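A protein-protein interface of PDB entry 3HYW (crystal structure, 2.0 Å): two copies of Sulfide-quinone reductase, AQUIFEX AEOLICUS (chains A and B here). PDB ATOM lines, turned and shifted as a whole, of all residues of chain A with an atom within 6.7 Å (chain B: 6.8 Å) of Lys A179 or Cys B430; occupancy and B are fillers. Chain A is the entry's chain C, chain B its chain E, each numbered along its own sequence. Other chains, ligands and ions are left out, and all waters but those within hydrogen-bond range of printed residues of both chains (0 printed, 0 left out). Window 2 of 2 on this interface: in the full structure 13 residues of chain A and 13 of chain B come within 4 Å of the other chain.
N of Tyr A178 is in hydrogen-bond range of OE1 of Glu B368 (3.0 Å).
The side-chain hydroxyl of Tyr A178 sits at hydrogen-bond distance from the side-chain carboxylate of Glu B417 (2.8 Å).
NE of Arg B429 lies within hydrogen-bond range of O of Tyr A178 (2.7 Å).
The chain-end carboxylate of Cys B430 lies within salt-bridge range of the side-chain amino group of Lys A179, 3.2 Å away.
The guanidinium group (NH2) of Arg A177 is in hydrogen-bond range of the backbone carbonyl oxygen (O) of Val A180 (2.8 Å).
NH1 of Arg B279 lies within hydrogen-bond range of O of Arg B429, at 3.3 Å.
The backbone carbonyl oxygen of Ala B340 is in hydrogen-bond range of the backbone NH of Glu B417.
The backbone carbonyl oxygen of Pro B366 is in hydrogen-bond range of the guanidinium group of Arg B429, at 2.6 Å.
SG of Cys B419 forms a disulfide with SG of Cys B430 (2.1 Å).
The side-chain sulfur (SG) of Cys B280 forms a disulfide with the side-chain sulfur (SG) of Cys B422 (2.0 Å).
CA of Gly A175 touches OE2 of Glu B368, at 3.7 Å.
CB of Pro B366 touches NH2 of Arg A177, at 3.5 Å.
Arg B367 touches Arg A177.
Glu B368 touches Arg A177 (OE1 to N, 3.5 Å).
Pro B366 touches Tyr A178 (O to CA, 3.3 Å).
Pro B366 touches Val A180.
Pro B366 touches Pro A181 (CG to N, 3.5 Å).
Of the printed residues of chain B, Tyr A178 touches Pro B366, Glu B368, Glu B417 and Arg B429.
Printed residues of chain B within 4 Å of Lys A179: Cys B430 (3.2 Å).
Of the printed residues of chain B, Val A180 touches Pro B366.
Printed residues of chain B within 4 Å of Pro A181: Pro B366.
Of the printed residues of chain A, Arg B367 touches Arg A177.
Of the printed residues of chain A, Glu B368 touches Gly A175, Arg A177 and Tyr A178.
Cys B422 touches none of the printed residues of chain A.
Cys B430 touches one residue of chain A.
The nearest printed residue of chain A that does not touch Glu B417 is Lys A179 (5.2 Å).
Hydrophobic or aromatic side chains of chain B within 4 Å of the printed part of chain A: Pro B366.
Hydrophobic or aromatic side chains of chain A within 4 Å of the printed part of chain B: Tyr A178 and Pro A181.
Along chain A the printed residues that touch a printed residue of chain B span positions 175 to 181.
Among the printed residues, no Asp or Glu carboxylate lies within 4 Å of a Lys or Arg side-chain nitrogen of the other chain.
No position is printed for both chains.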
ATOM      1  N   PRO A 143      30.465  17.942  -7.310  1.00  0.00           N
ATOM      2  CA  PRO A 143      30.857  16.709  -7.995  1.00  0.00           C
ATOM      3  C   PRO A 143      31.160  16.925  -9.478  1.00  0.00           C
ATOM      4  O   PRO A 143      30.500  17.725 -10.146  1.00  0.00           O
ATOM      5  CB  PRO A 143      29.626  15.814  -7.829  1.00  0.00           C
ATOM      6  CG  PRO A 143      28.950  16.322  -6.613  1.00  0.00           C
ATOM      7  CD  PRO A 143      29.160  17.801  -6.639  1.00  0.00           C
ATOM      8  N   GLY A 144      32.176  16.219  -9.962  1.00  0.00           N
ATOM      9  CA  GLY A 144      32.561  16.214 -11.373  1.00  0.00           C
ATOM     10  C   GLY A 144      33.315  14.918 -11.624  1.00  0.00           C
ATOM     11  O   GLY A 144      33.487  14.133 -10.692  1.00  0.00           O
ATOM     12  N   PRO A 145      33.762  14.679 -12.877  1.00  0.00           N
ATOM     13  CA  PRO A 145      34.497  13.442 -13.189  1.00  0.00           C
ATOM     14  C   PRO A 145      35.819  13.275 -12.436  1.00  0.00           C
ATOM     15  O   PRO A 145      36.571  14.244 -12.247  1.00  0.00           O
ATOM     16  CB  PRO A 145      34.740  13.529 -14.702  1.00  0.00           C
ATOM     17  CG  PRO A 145      34.544  14.965 -15.058  1.00  0.00           C
ATOM     18  CD  PRO A 145      33.575  15.531 -14.066  1.00  0.00           C
ATOM     19  N   GLY A 175      26.147   9.782  -0.702  1.00  0.00           N
ATOM     20  CA  GLY A 175      25.001   9.741  -1.615  1.00  0.00           C
ATOM     21  C   GLY A 175      25.192  10.501  -2.917  1.00  0.00           C
ATOM     22  O   GLY A 175      24.213  10.893  -3.554  1.00  0.00           O
ATOM     23  N   ILE A 176      26.446  10.701  -3.322  1.00  0.00           N
ATOM     24  CA  ILE A 176      26.758  11.509  -4.508  1.00  0.00           C
ATOM     25  C   ILE A 176      27.551  10.759  -5.596  1.00  0.00           C
ATOM     26  O   ILE A 176      28.001  11.362  -6.580  1.00  0.00           O
ATOM     27  CB  ILE A 176      27.462  12.855  -4.139  1.00  0.00           C
ATOM     28  CG1 ILE A 176      28.798  12.612  -3.428  1.00  0.00           C
ATOM     29  CG2 ILE A 176      26.534  13.746  -3.296  1.00  0.00           C
ATOM     30  CD1 ILE A 176      29.728  13.822  -3.436  1.00  0.00           C
ATOM     31  N   ARG A 177      27.708   9.446  -5.418  1.00  0.00           N
ATOM     32  CA  ARG A 177      28.425   8.591  -6.376  1.00  0.00           C
ATOM     33  C   ARG A 177      27.818   8.673  -7.787  1.00  0.00           C
ATOM     34  O   ARG A 177      28.540   8.644  -8.787  1.00  0.00           O
ATOM     35  CB  ARG A 177      28.458   7.143  -5.844  1.00  0.00           C
ATOM     36  CG  ARG A 177      29.236   6.091  -6.653  1.00  0.00           C
ATOM     37  CD  ARG A 177      30.692   6.452  -6.933  1.00  0.00           C
ATOM     38  NE  ARG A 177      30.855   6.789  -8.341  1.00  0.00           N
ATOM     39  CZ  ARG A 177      31.212   5.936  -9.297  1.00  0.00           C
ATOM     40  NH1 ARG A 177      31.481   4.672  -9.017  1.00  0.00           N
ATOM     41  NH2 ARG A 177      31.302   6.360 -10.545  1.00  0.00           N
ATOM     42  N   TYR A 178      26.495   8.817  -7.855  1.00  0.00           N
ATOM     43  CA  TYR A 178      25.786   8.925  -9.132  1.00  0.00           C
ATOM     44  C   TYR A 178      26.015  10.265  -9.841  1.00  0.00           C
ATOM     45  O   TYR A 178      25.589  10.448 -10.983  1.00  0.00           O
ATOM     46  CB  TYR A 178      24.285   8.647  -8.947  1.00  0.00           C
ATOM     47  CG  TYR A 178      23.472   9.816  -8.439  1.00  0.00           C
ATOM     48  CD1 TYR A 178      22.536  10.446  -9.265  1.00  0.00           C
ATOM     49  CD2 TYR A 178      23.627  10.290  -7.137  1.00  0.00           C
ATOM     50  CE1 TYR A 178      21.773  11.518  -8.806  1.00  0.00           C
ATOM     51  CE2 TYR A 178      22.866  11.364  -6.668  1.00  0.00           C
ATOM     52  CZ  TYR A 178      21.950  11.973  -7.507  1.00  0.00           C
ATOM     53  OH  TYR A 178      21.199  13.030  -7.046  1.00  0.00           O
ATOM     54  N   LYS A 179      26.699  11.181  -9.155  1.00  0.00           N
ATOM     55  CA  LYS A 179      27.064  12.489  -9.705  1.00  0.00           C
ATOM     56  C   LYS A 179      28.556  12.559 -10.059  1.00  0.00           C
ATOM     57  O   LYS A 179      29.032  13.557 -10.599  1.00  0.00           O
ATOM     58  CB  LYS A 179      26.719  13.601  -8.705  1.00  0.00           C
ATOM     59  CG  LYS A 179      25.234  13.902  -8.562  1.00  0.00           C
ATOM     60  CD  LYS A 179      25.009  14.984  -7.511  1.00  0.00           C
ATOM     61  CE  LYS A 179      23.529  15.321  -7.329  1.00  0.00           C
ATOM     62  NZ  LYS A 179      22.881  15.916  -8.539  1.00  0.00           N
ATOM     63  N   VAL A 180      29.284  11.488  -9.757  1.00  0.00           N
ATOM     64  CA  VAL A 180      30.730  11.461  -9.944  1.00  0.00           C
ATOM     65  C   VAL A 180      31.163  10.283 -10.828  1.00  0.00           C
ATOM     66  O   VAL A 180      31.238   9.146 -10.356  1.00  0.00           O
ATOM     67  CB  VAL A 180      31.480  11.403  -8.589  1.00  0.00           C
ATOM     68  CG1 VAL A 180      32.981  11.380  -8.816  1.00  0.00           C
ATOM     69  CG2 VAL A 180      31.087  12.580  -7.692  1.00  0.00           C
ATOM     70  N   PRO A 181      31.422  10.547 -12.125  1.00  0.00           N
ATOM     71  CA  PRO A 181      32.033   9.497 -12.946  1.00  0.00           C
ATOM     72  C   PRO A 181      33.411   9.126 -12.407  1.00  0.00           C
ATOM     73  O   PRO A 181      34.119   9.983 -11.876  1.00  0.00           O
ATOM     74  CB  PRO A 181      32.145  10.144 -14.334  1.00  0.00           C
ATOM     75  CG  PRO A 181      31.152  11.269 -14.321  1.00  0.00           C
ATOM     76  CD  PRO A 181      31.144  11.767 -12.901  1.00  0.00           C
ATOM     77  N   ARG B 279      15.699  17.629 -18.510  1.00  0.00           N
ATOM     78  CA  ARG B 279      15.930  16.772 -17.346  1.00  0.00           C
ATOM     79  C   ARG B 279      14.621  16.405 -16.658  1.00  0.00           C
ATOM     80  O   ARG B 279      14.515  15.344 -16.047  1.00  0.00           O
ATOM     81  CB  ARG B 279      16.839  17.466 -16.337  1.00  0.00           C
ATOM     82  CG  ARG B 279      18.296  17.515 -16.734  1.00  0.00           C
ATOM     83  CD  ARG B 279      19.076  18.309 -15.722  1.00  0.00           C
ATOM     84  NE  ARG B 279      20.478  18.446 -16.101  1.00  0.00           N
ATOM     85  CZ  ARG B 279      21.205  19.536 -15.873  1.00  0.00           C
ATOM     86  NH1 ARG B 279      22.473  19.579 -16.250  1.00  0.00           N
ATOM     87  NH2 ARG B 279      20.661  20.587 -15.274  1.00  0.00           N
ATOM     88  N   CYS B 280      13.641  17.304 -16.772  1.00  0.00           N
ATOM     89  CA  CYS B 280      12.328  17.161 -16.141  1.00  0.00           C
ATOM     90  C   CYS B 280      11.307  16.534 -17.114  1.00  0.00           C
ATOM     91  O   CYS B 280      10.091  16.566 -16.881  1.00  0.00           O
ATOM     92  CB  CYS B 280      11.877  18.534 -15.611  1.00  0.00           C
ATOM     93  SG  CYS B 280      13.056  19.184 -14.364  1.00  0.00           S
ATOM     94  N   TYR B 339      10.698  18.187 -10.867  1.00  0.00           N
ATOM     95  CA  TYR B 339      11.287  16.886 -10.592  1.00  0.00           C
ATOM     96  C   TYR B 339      11.917  16.235 -11.808  1.00  0.00           C
ATOM     97  O   TYR B 339      11.420  16.352 -12.931  1.00  0.00           O
ATOM     98  CB  TYR B 339      10.249  15.940  -9.968  1.00  0.00           C
ATOM     99  CG  TYR B 339       9.756  16.403  -8.615  1.00  0.00           C
ATOM    100  CD1 TYR B 339      10.448  16.072  -7.449  1.00  0.00           C
ATOM    101  CD2 TYR B 339       8.604  17.191  -8.501  1.00  0.00           C
ATOM    102  CE1 TYR B 339      10.002  16.503  -6.199  1.00  0.00           C
ATOM    103  CE2 TYR B 339       8.146  17.625  -7.256  1.00  0.00           C
ATOM    104  CZ  TYR B 339       8.852  17.278  -6.111  1.00  0.00           C
ATOM    105  OH  TYR B 339       8.410  17.708  -4.877  1.00  0.00           O
ATOM    106  N   ALA B 340      13.020  15.542 -11.560  1.00  0.00           N
ATOM    107  CA  ALA B 340      13.618  14.666 -12.546  1.00  0.00           C
ATOM    108  C   ALA B 340      13.416  13.232 -12.065  1.00  0.00           C
ATOM    109  O   ALA B 340      13.509  12.962 -10.863  1.00  0.00           O
ATOM    110  CB  ALA B 340      15.099  14.982 -12.701  1.00  0.00           C
ATOM    111  N   PRO B 366      27.110   7.860 -14.134  1.00  0.00           N
ATOM    112  CA  PRO B 366      27.642   6.899 -13.159  1.00  0.00           C
ATOM    113  C   PRO B 366      26.575   6.357 -12.208  1.00  0.00           C
ATOM    114  O   PRO B 366      25.610   7.046 -11.880  1.00  0.00           O
ATOM    115  CB  PRO B 366      28.689   7.709 -12.395  1.00  0.00           C
ATOM    116  CG  PRO B 366      28.244   9.122 -12.525  1.00  0.00           C
ATOM    117  CD  PRO B 366      27.563   9.236 -13.853  1.00  0.00           C
ATOM    118  N   ARG B 367      26.773   5.122 -11.770  1.00  0.00           N
ATOM    119  CA  ARG B 367      25.792   4.408 -10.975  1.00  0.00           C
ATOM    120  C   ARG B 367      26.132   4.423  -9.492  1.00  0.00           C
ATOM    121  O   ARG B 367      27.304   4.384  -9.111  1.00  0.00           O
ATOM    122  CB  ARG B 367      25.675   2.967 -11.471  1.00  0.00           C
ATOM    123  CG  ARG B 367      25.515   2.856 -12.982  1.00  0.00           C
ATOM    124  CD  ARG B 367      24.698   1.652 -13.349  1.00  0.00           C
ATOM    125  NE  ARG B 367      24.322   1.657 -14.760  1.00  0.00           N
ATOM    126  CZ  ARG B 367      24.900   0.909 -15.692  1.00  0.00           C
ATOM    127  NH1 ARG B 367      24.479   0.981 -16.946  1.00  0.00           N
ATOM    128  NH2 ARG B 367      25.892   0.092 -15.375  1.00  0.00           N
ATOM    129  N   GLU B 368      25.093   4.480  -8.668  1.00  0.00           N
ATOM    130  CA  GLU B 368      25.215   4.349  -7.224  1.00  0.00           C
ATOM    131  C   GLU B 368      25.454   2.884  -6.880  1.00  0.00           C
ATOM    132  O   GLU B 368      26.346   2.568  -6.101  1.00  0.00           O
ATOM    133  CB  GLU B 368      23.940   4.859  -6.538  1.00  0.00           C
ATOM    134  CG  GLU B 368      24.109   5.265  -5.076  1.00  0.00           C
ATOM    135  CD  GLU B 368      24.842   6.591  -4.894  1.00  0.00           C
ATOM    136  OE1 GLU B 368      24.826   7.435  -5.818  1.00  0.00           O
ATOM    137  OE2 GLU B 368      25.434   6.795  -3.810  1.00  0.00           O
ATOM    138  N   GLU B 417      13.536  12.996  -8.019  1.00  0.00           N
ATOM    139  CA  GLU B 417      14.315  13.939  -7.213  1.00  0.00           C
ATOM    140  C   GLU B 417      13.952  15.363  -7.584  1.00  0.00           C
ATOM    141  O   GLU B 417      13.661  15.658  -8.743  1.00  0.00           O
ATOM    142  CB  GLU B 417      15.816  13.743  -7.432  1.00  0.00           C
ATOM    143  CG  GLU B 417      16.298  12.288  -7.404  1.00  0.00           C
ATOM    144  CD  GLU B 417      17.808  12.150  -7.525  1.00  0.00           C
ATOM    145  OE1 GLU B 417      18.497  13.140  -7.892  1.00  0.00           O
ATOM    146  OE2 GLU B 417      18.315  11.044  -7.240  1.00  0.00           O
ATOM    147  N   LEU B 418      13.987  16.240  -6.588  1.00  0.00           N
ATOM    148  CA  LEU B 418      13.871  17.668  -6.809  1.00  0.00           C
ATOM    149  C   LEU B 418      14.991  18.098  -7.750  1.00  0.00           C
ATOM    150  O   LEU B 418      16.159  17.768  -7.525  1.00  0.00           O
ATOM    151  CB  LEU B 418      13.989  18.401  -5.473  1.00  0.00           C
ATOM    152  CG  LEU B 418      13.252  19.724  -5.293  1.00  0.00           C
ATOM    153  CD1 LEU B 418      11.780  19.556  -5.608  1.00  0.00           C
ATOM    154  CD2 LEU B 418      13.448  20.233  -3.863  1.00  0.00           C
ATOM    155  N   CYS B 419      14.624  18.792  -8.825  1.00  0.00           N
ATOM    156  CA  CYS B 419      15.599  19.264  -9.802  1.00  0.00           C
ATOM    157  C   CYS B 419      15.687  20.786  -9.801  1.00  0.00           C
ATOM    158  O   CYS B 419      14.742  21.468 -10.198  1.00  0.00           O
ATOM    159  CB  CYS B 419      15.257  18.745 -11.200  1.00  0.00           C
ATOM    160  SG  CYS B 419      16.496  19.128 -12.449  1.00  0.00           S
ATOM    161  N   LYS B 420      16.831  21.307  -9.361  1.00  0.00           N
ATOM    162  CA  LYS B 420      17.047  22.755  -9.246  1.00  0.00           C
ATOM    163  C   LYS B 420      17.162  23.474 -10.598  1.00  0.00           C
ATOM    164  O   LYS B 420      16.964  24.689 -10.678  1.00  0.00           O
ATOM    165  CB  LYS B 420      18.285  23.050  -8.385  1.00  0.00           C
ATOM    166  CG  LYS B 420      19.578  22.420  -8.892  1.00  0.00           C
ATOM    167  CD  LYS B 420      20.805  23.043  -8.245  1.00  0.00           C
ATOM    168  CE  LYS B 420      21.160  22.375  -6.921  1.00  0.00           C
ATOM    169  NZ  LYS B 420      22.474  22.885  -6.413  1.00  0.00           N
ATOM    170  N   ASP B 421      17.489  22.717 -11.643  1.00  0.00           N
ATOM    171  CA  ASP B 421      17.709  23.248 -12.985  1.00  0.00           C
ATOM    172  C   ASP B 421      17.389  22.151 -14.003  1.00  0.00           C
ATOM    173  O   ASP B 421      18.174  21.225 -14.200  1.00  0.00           O
ATOM    174  CB  ASP B 421      19.167  23.717 -13.124  1.00  0.00           C
ATOM    175  CG  ASP B 421      19.461  24.398 -14.458  1.00  0.00           C
ATOM    176  OD1 ASP B 421      18.538  24.587 -15.281  1.00  0.00           O
ATOM    177  OD2 ASP B 421      20.641  24.756 -14.679  1.00  0.00           O
ATOM    178  N   CYS B 422      16.219  22.260 -14.628  1.00  0.00           N
ATOM    179  CA  CYS B 422      15.756  21.290 -15.620  1.00  0.00           C
ATOM    180  C   CYS B 422      16.572  21.344 -16.913  1.00  0.00           C
ATOM    181  O   CYS B 422      16.576  20.383 -17.685  1.00  0.00           O
ATOM    182  CB  CYS B 422      14.271  21.512 -15.945  1.00  0.00           C
ATOM    183  SG  CYS B 422      13.082  21.206 -14.596  1.00  0.00           S
ATOM    184  N   GLU B 423      17.256  22.466 -17.148  1.00  0.00           N
ATOM    185  CA  GLU B 423      18.001  22.674 -18.393  1.00  0.00           C
ATOM    186  C   GLU B 423      19.145  21.689 -18.584  1.00  0.00           C
ATOM    187  O   GLU B 423      20.181  21.778 -17.923  1.00  0.00           O
ATOM    188  CB  GLU B 423      18.522  24.110 -18.505  1.00  0.00           C
ATOM    189  CG  GLU B 423      17.439  25.146 -18.744  1.00  0.00           C
ATOM    190  CD  GLU B 423      17.995  26.458 -19.285  1.00  0.00           C
ATOM    191  OE1 GLU B 423      18.828  26.411 -20.215  1.00  0.00           O
ATOM    192  OE2 GLU B 423      17.588  27.532 -18.783  1.00  0.00           O
ATOM    193  N   SER B 428      20.765  13.481 -17.484  1.00  0.00           N
ATOM    194  CA  SER B 428      21.899  14.236 -16.939  1.00  0.00           C
ATOM    195  C   SER B 428      21.537  14.806 -15.569  1.00  0.00           C
ATOM    196  O   SER B 428      20.363  15.037 -15.278  1.00  0.00           O
ATOM    197  CB  SER B 428      22.363  15.346 -17.895  1.00  0.00           C
ATOM    198  OG  SER B 428      21.401  16.374 -18.018  1.00  0.00           O
ATOM    199  N   ARG B 429      22.545  15.044 -14.738  1.00  0.00           N
ATOM    200  CA  ARG B 429      22.314  15.373 -13.336  1.00  0.00           C
ATOM    201  C   ARG B 429      22.159  16.871 -13.107  1.00  0.00           C
ATOM    202  O   ARG B 429      22.968  17.660 -13.603  1.00  0.00           O
ATOM    203  CB  ARG B 429      23.445  14.809 -12.469  1.00  0.00           C
ATOM    204  CG  ARG B 429      23.253  13.359 -12.014  1.00  0.00           C
ATOM    205  CD  ARG B 429      23.107  12.369 -13.169  1.00  0.00           C
ATOM    206  NE  ARG B 429      23.714  11.084 -12.841  1.00  0.00           N
ATOM    207  CZ  ARG B 429      23.511   9.947 -13.496  1.00  0.00           C
ATOM    208  NH1 ARG B 429      22.693   9.896 -14.543  1.00  0.00           N
ATOM    209  NH2 ARG B 429      24.132   8.849 -13.093  1.00  0.00           N
ATOM    210  N   CYS B 430      21.117  17.245 -12.355  1.00  0.00           N
ATOM    211  CA  CYS B 430      20.857  18.645 -11.980  1.00  0.00           C
ATOM    212  C   CYS B 430      21.929  19.108 -10.984  1.00  0.00           C
ATOM    213  O   CYS B 430      22.808  18.338 -10.580  1.00  0.00           O
ATOM    214  CB  CYS B 430      19.432  18.841 -11.382  1.00  0.00           C
ATOM    215  SG  CYS B 430      18.026  17.815 -12.072  1.00  0.00           S
ATOM    216  OXT CYS B 430      21.962  20.259 -10.547  1.00  0.00           O
